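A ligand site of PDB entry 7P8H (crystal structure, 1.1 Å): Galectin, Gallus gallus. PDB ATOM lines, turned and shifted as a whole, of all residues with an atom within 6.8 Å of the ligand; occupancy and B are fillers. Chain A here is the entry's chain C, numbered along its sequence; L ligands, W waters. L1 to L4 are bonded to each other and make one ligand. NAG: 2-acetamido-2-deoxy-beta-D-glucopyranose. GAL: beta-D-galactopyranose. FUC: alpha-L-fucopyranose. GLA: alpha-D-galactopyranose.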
ATOM      1  N   MET A  31       0.899  21.014  15.135  1.00  0.00           N
ATOM      2  CA  MET A  31       0.858  20.239  13.897  1.00  0.00           C
ATOM      3  C   MET A  31      -0.589  20.130  13.459  1.00  0.00           C
ATOM      4  O   MET A  31      -1.507  20.354  14.248  1.00  0.00           O
ATOM      5  CB  MET A  31       1.460  18.854  14.085  1.00  0.00           C
ATOM      6  CG  MET A  31       0.744  18.001  15.106  1.00  0.00           C
ATOM      7  SD  MET A  31       1.455  16.357  15.256  1.00  0.00           S
ATOM      8  CE  MET A  31       3.063  16.735  15.947  1.00  0.00           C
ATOM      9  N   GLU A  33      -3.128  17.678  10.453  1.00  0.00           N
ATOM     10  CA  GLU A  33      -3.116  16.576   9.513  1.00  0.00           C
ATOM     11  C   GLU A  33      -4.309  16.651   8.574  1.00  0.00           C
ATOM     12  O   GLU A  33      -5.392  17.117   8.945  1.00  0.00           O
ATOM     13  CB  GLU A  33      -3.029  15.211  10.194  1.00  0.00           C
ATOM     14  CG  GLU A  33      -4.135  14.941  11.162  1.00  0.00           C
ATOM     15  CD  GLU A  33      -3.831  13.770  12.052  1.00  0.00           C
ATOM     16  OE1 GLU A  33      -2.953  13.873  12.918  1.00  0.00           O
ATOM     17  OE2 GLU A  33      -4.421  12.691  11.847  1.00  0.00           O
ATOM     18  N   ASN A  35      -6.186  13.783   6.288  1.00  0.00           N
ATOM     19  CA  ASN A  35      -6.304  12.344   6.113  1.00  0.00           C
ATOM     20  C   ASN A  35      -7.348  12.023   5.062  1.00  0.00           C
ATOM     21  O   ASN A  35      -8.449  12.599   5.056  1.00  0.00           O
ATOM     22  CB  ASN A  35      -6.722  11.686   7.417  1.00  0.00           C
ATOM     23  CG  ASN A  35      -5.694  11.856   8.500  1.00  0.00           C
ATOM     24  OD1 ASN A  35      -4.501  11.847   8.267  1.00  0.00           O
ATOM     25  ND2 ASN A  35      -6.173  12.014   9.729  1.00  0.00           N
ATOM     26  N   ILE A  44      -6.701   4.752   7.040  1.00  0.00           N
ATOM     27  CA  ILE A  44      -6.162   6.013   6.551  1.00  0.00           C
ATOM     28  C   ILE A  44      -5.274   5.697   5.349  1.00  0.00           C
ATOM     29  O   ILE A  44      -4.124   5.263   5.490  1.00  0.00           O
ATOM     30  CB  ILE A  44      -5.408   6.815   7.617  1.00  0.00           C
ATOM     31  CG1 ILE A  44      -6.309   7.054   8.843  1.00  0.00           C
ATOM     32  CG2 ILE A  44      -4.952   8.128   6.998  1.00  0.00           C
ATOM     33  CD1 ILE A  44      -5.619   7.768   9.988  1.00  0.00           C
ATOM     34  N   HIS A  47      -2.117   9.966   5.067  1.00  0.00           N
ATOM     35  CA  HIS A  47      -1.996  10.846   6.228  1.00  0.00           C
ATOM     36  C   HIS A  47      -0.885  11.832   5.883  1.00  0.00           C
ATOM     37  O   HIS A  47       0.266  11.417   5.673  1.00  0.00           O
ATOM     38  CB  HIS A  47      -1.613   9.964   7.422  1.00  0.00           C
ATOM     39  CG  HIS A  47      -1.224  10.679   8.698  1.00  0.00           C
ATOM     40  ND1 HIS A  47      -2.118  11.333   9.511  1.00  0.00           N
ATOM     41  CD2 HIS A  47      -0.045  10.655   9.373  1.00  0.00           C
ATOM     42  CE1 HIS A  47      -1.490  11.740  10.608  1.00  0.00           C
ATOM     43  NE2 HIS A  47      -0.239  11.333  10.543  1.00  0.00           N
ATOM     44  N   ASN A  49       0.921  15.086   7.390  1.00  0.00           N
ATOM     45  CA  ASN A  49       1.058  15.595   8.766  1.00  0.00           C
ATOM     46  C   ASN A  49       2.232  16.546   8.896  1.00  0.00           C
ATOM     47  O   ASN A  49       3.336  16.149   9.292  1.00  0.00           O
ATOM     48  CB  ASN A  49       1.184  14.389   9.709  1.00  0.00           C
ATOM     49  CG  ASN A  49       1.367  14.736  11.182  1.00  0.00           C
ATOM     50  OD1 ASN A  49       1.966  13.950  11.917  1.00  0.00           O
ATOM     51  ND2 ASN A  49       0.809  15.853  11.641  1.00  0.00           N
ATOM     52  N   ARG A  51       4.462  18.961  10.804  1.00  0.00           N
ATOM     53  CA  ARG A  51       4.815  19.121  12.213  1.00  0.00           C
ATOM     54  C   ARG A  51       5.689  20.356  12.349  1.00  0.00           C
ATOM     55  O   ARG A  51       6.842  20.377  11.902  1.00  0.00           O
ATOM     56  CB  ARG A  51       5.518  17.857  12.711  1.00  0.00           C
ATOM     57  CG  ARG A  51       4.651  16.613  12.592  1.00  0.00           C
ATOM     58  CD  ARG A  51       5.374  15.408  13.127  1.00  0.00           C
ATOM     59  NE  ARG A  51       4.546  14.216  12.994  1.00  0.00           N
ATOM     60  CZ  ARG A  51       4.946  13.000  13.339  1.00  0.00           C
ATOM     61  NH1 ARG A  51       6.140  12.790  13.850  1.00  0.00           N
ATOM     62  NH2 ARG A  51       4.120  11.981  13.155  1.00  0.00           N
ATOM     63  N   ARG A  56       8.949  19.230   9.893  1.00  0.00           N
ATOM     64  CA  ARG A  56       8.947  18.007   9.102  1.00  0.00           C
ATOM     65  C   ARG A  56       7.523  17.703   8.653  1.00  0.00           C
ATOM     66  O   ARG A  56       6.593  17.761   9.463  1.00  0.00           O
ATOM     67  CB  ARG A  56       9.466  16.820   9.919  1.00  0.00           C
ATOM     68  CG  ARG A  56      10.930  16.947  10.309  1.00  0.00           C
ATOM     69  CD  ARG A  56      11.319  16.049  11.491  1.00  0.00           C
ATOM     70  NE  ARG A  56      11.772  14.731  11.065  1.00  0.00           N
ATOM     71  CZ  ARG A  56      11.078  13.605  11.194  1.00  0.00           C
ATOM     72  NH1 ARG A  56       9.867  13.594  11.737  1.00  0.00           N
ATOM     73  NH2 ARG A  56      11.613  12.458  10.779  1.00  0.00           N
ATOM     74  N   VAL A  58       5.422  14.653   7.690  1.00  0.00           N
ATOM     75  CA  VAL A  58       5.368  13.198   7.776  1.00  0.00           C
ATOM     76  C   VAL A  58       4.154  12.697   6.989  1.00  0.00           C
ATOM     77  O   VAL A  58       3.027  13.139   7.229  1.00  0.00           O
ATOM     78  CB  VAL A  58       5.293  12.740   9.244  1.00  0.00           C
ATOM     79  CG1 VAL A  58       5.175  11.233   9.329  1.00  0.00           C
ATOM     80  CG2 VAL A  58       6.522  13.258  10.034  1.00  0.00           C
ATOM     81  N   CYS A  59       4.382  11.755   6.076  1.00  0.00           N
ATOM     82  CA  CYS A  59       3.331  11.088   5.316  1.00  0.00           C
ATOM     83  C   CYS A  59       3.364   9.598   5.614  1.00  0.00           C
ATOM     84  O   CYS A  59       4.426   9.005   5.742  1.00  0.00           O
ATOM     85  CB  CYS A  59       3.510  11.320   3.818  1.00  0.00           C
ATOM     86  SG  CYS A  59       3.259  13.016   3.292  1.00  0.00           S
ATOM     87  N   ASN A  60       2.183   8.991   5.724  1.00  0.00           N
ATOM     88  CA  ASN A  60       2.090   7.571   6.035  1.00  0.00           C
ATOM     89  C   ASN A  60       0.667   7.112   5.721  1.00  0.00           C
ATOM     90  O   ASN A  60      -0.180   7.892   5.274  1.00  0.00           O
ATOM     91  CB  ASN A  60       2.461   7.377   7.519  1.00  0.00           C
ATOM     92  CG  ASN A  60       3.025   5.991   7.825  1.00  0.00           C
ATOM     93  OD1 ASN A  60       2.916   5.051   7.024  1.00  0.00           O
ATOM     94  ND2 ASN A  60       3.647   5.871   8.984  1.00  0.00           N
ATOM     95  N   SER A  61       0.437   5.813   5.942  1.00  0.00           N
ATOM     96  CA  SER A  61      -0.863   5.189   5.836  1.00  0.00           C
ATOM     97  C   SER A  61      -1.084   4.334   7.070  1.00  0.00           C
ATOM     98  O   SER A  61      -0.147   3.766   7.634  1.00  0.00           O
ATOM     99  CB  SER A  61      -0.955   4.294   4.590  1.00  0.00           C
ATOM    100  OG  SER A  61      -0.665   5.016   3.410  1.00  0.00           O
ATOM    101  N   PHE A  62      -2.338   4.261   7.498  1.00  0.00           N
ATOM    102  CA  PHE A  62      -2.774   3.429   8.622  1.00  0.00           C
ATOM    103  C   PHE A  62      -3.698   2.352   8.065  1.00  0.00           C
ATOM    104  O   PHE A  62      -4.888   2.610   7.804  1.00  0.00           O
ATOM    105  CB  PHE A  62      -3.472   4.250   9.700  1.00  0.00           C
ATOM    106  CG  PHE A  62      -3.732   3.477  10.962  1.00  0.00           C
ATOM    107  CD1 PHE A  62      -2.733   3.289  11.891  1.00  0.00           C
ATOM    108  CD2 PHE A  62      -4.988   2.971  11.228  1.00  0.00           C
ATOM    109  CE1 PHE A  62      -2.959   2.592  13.056  1.00  0.00           C
ATOM    110  CE2 PHE A  62      -5.227   2.256  12.390  1.00  0.00           C
ATOM    111  CZ  PHE A  62      -4.211   2.078  13.315  1.00  0.00           C
ATOM    112  N   TRP A  67       0.373   1.762  11.510  1.00  0.00           N
ATOM    113  CA  TRP A  67       1.082   2.726  10.669  1.00  0.00           C
ATOM    114  C   TRP A  67       2.200   2.010   9.902  1.00  0.00           C
ATOM    115  O   TRP A  67       2.862   1.134  10.443  1.00  0.00           O
ATOM    116  CB  TRP A  67       1.691   3.843  11.524  1.00  0.00           C
ATOM    117  CG  TRP A  67       0.674   4.784  12.036  1.00  0.00           C
ATOM    118  CD1 TRP A  67       0.224   4.885  13.319  1.00  0.00           C
ATOM    119  CD2 TRP A  67      -0.070   5.745  11.271  1.00  0.00           C
ATOM    120  NE1 TRP A  67      -0.743   5.859  13.402  1.00  0.00           N
ATOM    121  CE2 TRP A  67      -0.944   6.406  12.154  1.00  0.00           C
ATOM    122  CE3 TRP A  67      -0.074   6.107   9.922  1.00  0.00           C
ATOM    123  CZ2 TRP A  67      -1.815   7.409  11.734  1.00  0.00           C
ATOM    124  CZ3 TRP A  67      -0.941   7.102   9.496  1.00  0.00           C
ATOM    125  CH2 TRP A  67      -1.795   7.754  10.401  1.00  0.00           C
ATOM    126  N   GLY A  68       2.394   2.394   8.646  1.00  0.00           N
ATOM    127  CA  GLY A  68       3.471   1.868   7.833  1.00  0.00           C
ATOM    128  C   GLY A  68       4.739   2.671   7.981  1.00  0.00           C
ATOM    129  O   GLY A  68       4.982   3.323   9.004  1.00  0.00           O
ATOM    130  N   LYS A  69       5.576   2.612   6.952  1.00  0.00           N
ATOM    131  CA  LYS A  69       6.833   3.349   6.956  1.00  0.00           C
ATOM    132  C   LYS A  69       6.596   4.821   6.694  1.00  0.00           C
ATOM    133  O   LYS A  69       5.903   5.202   5.745  1.00  0.00           O
ATOM    134  CB  LYS A  69       7.765   2.777   5.885  1.00  0.00           C
ATOM    135  CG  LYS A  69       9.144   3.434   5.885  1.00  0.00           C
ATOM    136  CD  LYS A  69      10.091   2.792   4.879  1.00  0.00           C
ATOM    137  CE  LYS A  69      11.521   3.318   5.042  1.00  0.00           C
ATOM    138  NZ  LYS A  69      12.463   2.784   4.013  1.00  0.00           N
ATOM    139  N   GLU A  70       7.179   5.680   7.525  1.00  0.00           N
ATOM    140  CA  GLU A  70       7.030   7.114   7.324  1.00  0.00           C
ATOM    141  C   GLU A  70       7.830   7.561   6.117  1.00  0.00           C
ATOM    142  O   GLU A  70       8.961   7.120   5.913  1.00  0.00           O
ATOM    143  CB  GLU A  70       7.508   7.865   8.566  1.00  0.00           C
ATOM    144  CG  GLU A  70       6.579   7.693   9.743  1.00  0.00           C
ATOM    145  CD  GLU A  70       6.934   8.518  10.962  1.00  0.00           C
ATOM    146  OE1 GLU A  70       8.076   9.027  11.063  1.00  0.00           O
ATOM    147  OE2 GLU A  70       6.050   8.676  11.820  1.00  0.00           O
ATOM    148  N   ASN A 124      -6.647  19.252  13.914  1.00  0.00           N
ATOM    149  CA  ASN A 124      -5.642  19.884  14.763  1.00  0.00           C
ATOM    150  C   ASN A 124      -5.317  21.306  14.331  1.00  0.00           C
ATOM    151  O   ASN A 124      -6.249  22.059  14.046  1.00  0.00           O
ATOM    152  CB  ASN A 124      -4.469  18.919  14.986  1.00  0.00           C
ATOM    153  CG  ASN A 124      -4.917  17.654  15.666  1.00  0.00           C
ATOM    154  OD1 ASN A 124      -5.844  17.687  16.474  1.00  0.00           O
ATOM    155  ND2 ASN A 124      -4.307  16.535  15.307  1.00  0.00           N
HETATM  156  C1  NAG L   1       6.901   6.640  16.345  1.00  0.00           C
HETATM  157  C2  NAG L   1       5.608   7.410  16.640  1.00  0.00           C
HETATM  158  C3  NAG L   1       5.271   8.275  15.390  1.00  0.00           C
HETATM  159  C4  NAG L   1       6.473   9.224  15.193  1.00  0.00           C
HETATM  160  C5  NAG L   1       7.746   8.329  14.997  1.00  0.00           C
HETATM  161  C6  NAG L   1       8.969   9.187  14.775  1.00  0.00           C
HETATM  162  C7  NAG L   1       4.237   6.078  18.244  1.00  0.00           C
HETATM  163  C8  NAG L   1       4.963   6.750  19.410  1.00  0.00           C
HETATM  164  N2  NAG L   1       4.566   6.428  16.930  1.00  0.00           N
HETATM  165  O1  NAG L   1       7.190   5.945  17.504  1.00  0.00           O
HETATM  166  O3  NAG L   1       4.149   9.036  15.649  1.00  0.00           O
HETATM  167  O4  NAG L   1       6.267   9.998  14.027  1.00  0.00           O
HETATM  168  O5  NAG L   1       7.937   7.569  16.190  1.00  0.00           O
HETATM  169  O6  NAG L   1       9.039  10.121  15.804  1.00  0.00           O
HETATM  170  O7  NAG L   1       3.380   5.252  18.498  1.00  0.00           O
HETATM  171  C1  GAL L   2       2.995   8.672  14.975  1.00  0.00           C
HETATM  172  C2  GAL L   2       1.846   9.553  15.528  1.00  0.00           C
HETATM  173  C3  GAL L   2       0.597   9.304  14.654  1.00  0.00           C
HETATM  174  C4  GAL L   2       0.940   9.502  13.133  1.00  0.00           C
HETATM  175  C5  GAL L   2       2.144   8.584  12.794  1.00  0.00           C
HETATM  176  C6  GAL L   2       2.585   8.781  11.377  1.00  0.00           C
HETATM  177  O2  GAL L   2       1.611   9.095  16.860  1.00  0.00           O
HETATM  178  O3  GAL L   2      -0.383  10.182  15.113  1.00  0.00           O
HETATM  179  O4  GAL L   2       1.228  10.852  12.877  1.00  0.00           O
HETATM  180  O5  GAL L   2       3.231   8.972  13.626  1.00  0.00           O
HETATM  181  O6  GAL L   2       3.604   7.855  11.071  1.00  0.00           O
HETATM  182  C1  FUC L   3       1.302  10.112  17.805  1.00  0.00           C
HETATM  183  C2  FUC L   3       0.782   9.497  19.119  1.00  0.00           C
HETATM  184  C3  FUC L   3       1.888   8.597  19.773  1.00  0.00           C
HETATM  185  C4  FUC L   3       3.112   9.491  20.020  1.00  0.00           C
HETATM  186  C5  FUC L   3       3.568  10.127  18.662  1.00  0.00           C
HETATM  187  C6  FUC L   3       4.809  10.989  18.770  1.00  0.00           C
HETATM  188  O2  FUC L   3      -0.269   8.660  18.786  1.00  0.00           O
HETATM  189  O3  FUC L   3       1.399   8.128  20.982  1.00  0.00           O
HETATM  190  O4  FUC L   3       2.844  10.511  20.948  1.00  0.00           O
HETATM  191  O5  FUC L   3       2.502  10.864  18.069  1.00  0.00           O
HETATM  192  C1  GLA L   4      -1.683   9.980  14.564  1.00  0.00           C
HETATM  193  C2  GLA L   4      -2.674  10.992  15.118  1.00  0.00           C
HETATM  194  C3  GLA L   4      -2.806  10.768  16.648  1.00  0.00           C
HETATM  195  C4  GLA L   4      -3.257   9.291  16.896  1.00  0.00           C
HETATM  196  C5  GLA L   4      -2.251   8.339  16.220  1.00  0.00           C
HETATM  197  C6  GLA L   4      -2.630   6.859  16.408  1.00  0.00           C
HETATM  198  O2  GLA L   4      -2.182  12.257  14.840  1.00  0.00           O
HETATM  199  O3  GLA L   4      -3.775  11.659  17.147  1.00  0.00           O
HETATM  200  O4  GLA L   4      -4.528   9.060  16.367  1.00  0.00           O
HETATM  201  O5  GLA L   4      -2.110   8.640  14.854  1.00  0.00           O
HETATM  202  O6  GLA L   4      -1.564   6.025  16.058  1.00  0.00           O
HETATM  203  O   HOH W   1      -6.456  11.017  15.901  1.00  0.00           O
HETATM  204  O   HOH W   2       4.326   5.696  12.878  1.00  0.00           O
HETATM  205  O   HOH W   3       4.769   9.682  22.839  1.00  0.00           O
HETATM  206  O   HOH W   4       0.264   6.234  17.671  1.00  0.00           O
HETATM  207  O   HOH W   5      -0.977   2.892  16.320  1.00  0.00           O
HETATM  208  O   HOH W   6       3.452   4.924  15.156  1.00  0.00           O
HETATM  209  O   HOH W   7      -2.209   9.371  21.087  1.00  0.00           O
HETATM  210  O   HOH W   8      -0.573  13.726  16.372  1.00  0.00           O
HETATM  211  O   HOH W   9      -4.980   8.364  13.722  1.00  0.00           O
HETATM  212  O   HOH W  10       1.220  13.103  14.515  1.00  0.00           O
HETATM  213  O   HOH W  11       0.541   5.572  21.450  1.00  0.00           O
HETATM  214  O   HOH W  12       3.033  13.241  16.643  1.00  0.00           O
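An oxygen (O6) of GAL L2 is in hydrogen-bond range of the side-chain amide nitrogen (ND2) of Asn 60, 2.9 Å away.
A ring nitrogen (NE2) of His 47 lies within hydrogen-bond range of an oxygen (O4) of GAL L2, 2.8 Å away.
NH1 of Arg 51 is in hydrogen-bond range of O4 of NAG L1.
The side-chain carboxylate (OE2) of Glu 70 sits at hydrogen-bond distance from an oxygen (O4) of NAG L1 (2.6 Å).
An oxygen (O6) of GLA L4 lies within hydrogen-bond range of the indole nitrogen of Trp 67 (2.8 Å).
The side-chain carboxylate of Glu 33 sits at hydrogen-bond distance from an oxygen (O2) of GLA L4, 2.6 Å away.
OD1 of Asn 49 sits at hydrogen-bond distance from O4 of GAL L2 (3.3 Å).
The side-chain amide nitrogen (ND2) of Asn 49 lies within hydrogen-bond range of the side-chain sulfur (SD) of Met 31.
The backbone NH of Asn 49 sits at hydrogen-bond distance from the backbone carbonyl oxygen of Val 58.
The backbone carbonyl oxygen (O) of Asn 60 is in hydrogen-bond range of the backbone NH (N) of His 47 (2.8 Å).
OD1 of Asn 60 sits close to O of Lys 69.
The side-chain amide oxygen (OD1) of Asn 49 is in hydrogen-bond range of the guanidinium group (NE) of Arg 51.
O of Gly 68 lies within hydrogen-bond range of ND2 of Asn 60, at 2.9 Å.
OE2 of Glu 33 is in hydrogen-bond range of ND2 of Asn 35 (2.8 Å).
A ring nitrogen (ND1) of His 47 is in hydrogen-bond range of the side-chain amide oxygen (OD1) of Asn 35 (2.7 Å).
Hydrophobic or aromatic side chains within 4 Å of the ligand: His 47 and Trp 67.
Within 4 Å of the ligand: Glu 33, His 47, Asn 49, Arg 51, Asn 60, Trp 67 and Glu 70.
Water W8 lies within hydrogen-bond range of an oxygen (O2) of GLA L4 (2.7 Å) and the side-chain sulfur (SD) of Met 31 (3.5 Å).
Water W10 lies within hydrogen-bond range of an oxygen (O4) of GAL L2 (2.8 Å), the side-chain amide oxygen of Asn 49 (2.8 Å), the side-chain sulfur of Met 31 (3.3 Å) and the guanidinium group of Arg 51 (3.4 Å).
Water W12 bridges O5 of FUC L3 (2.8 Å) and SD of Met 31 (3.8 Å).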
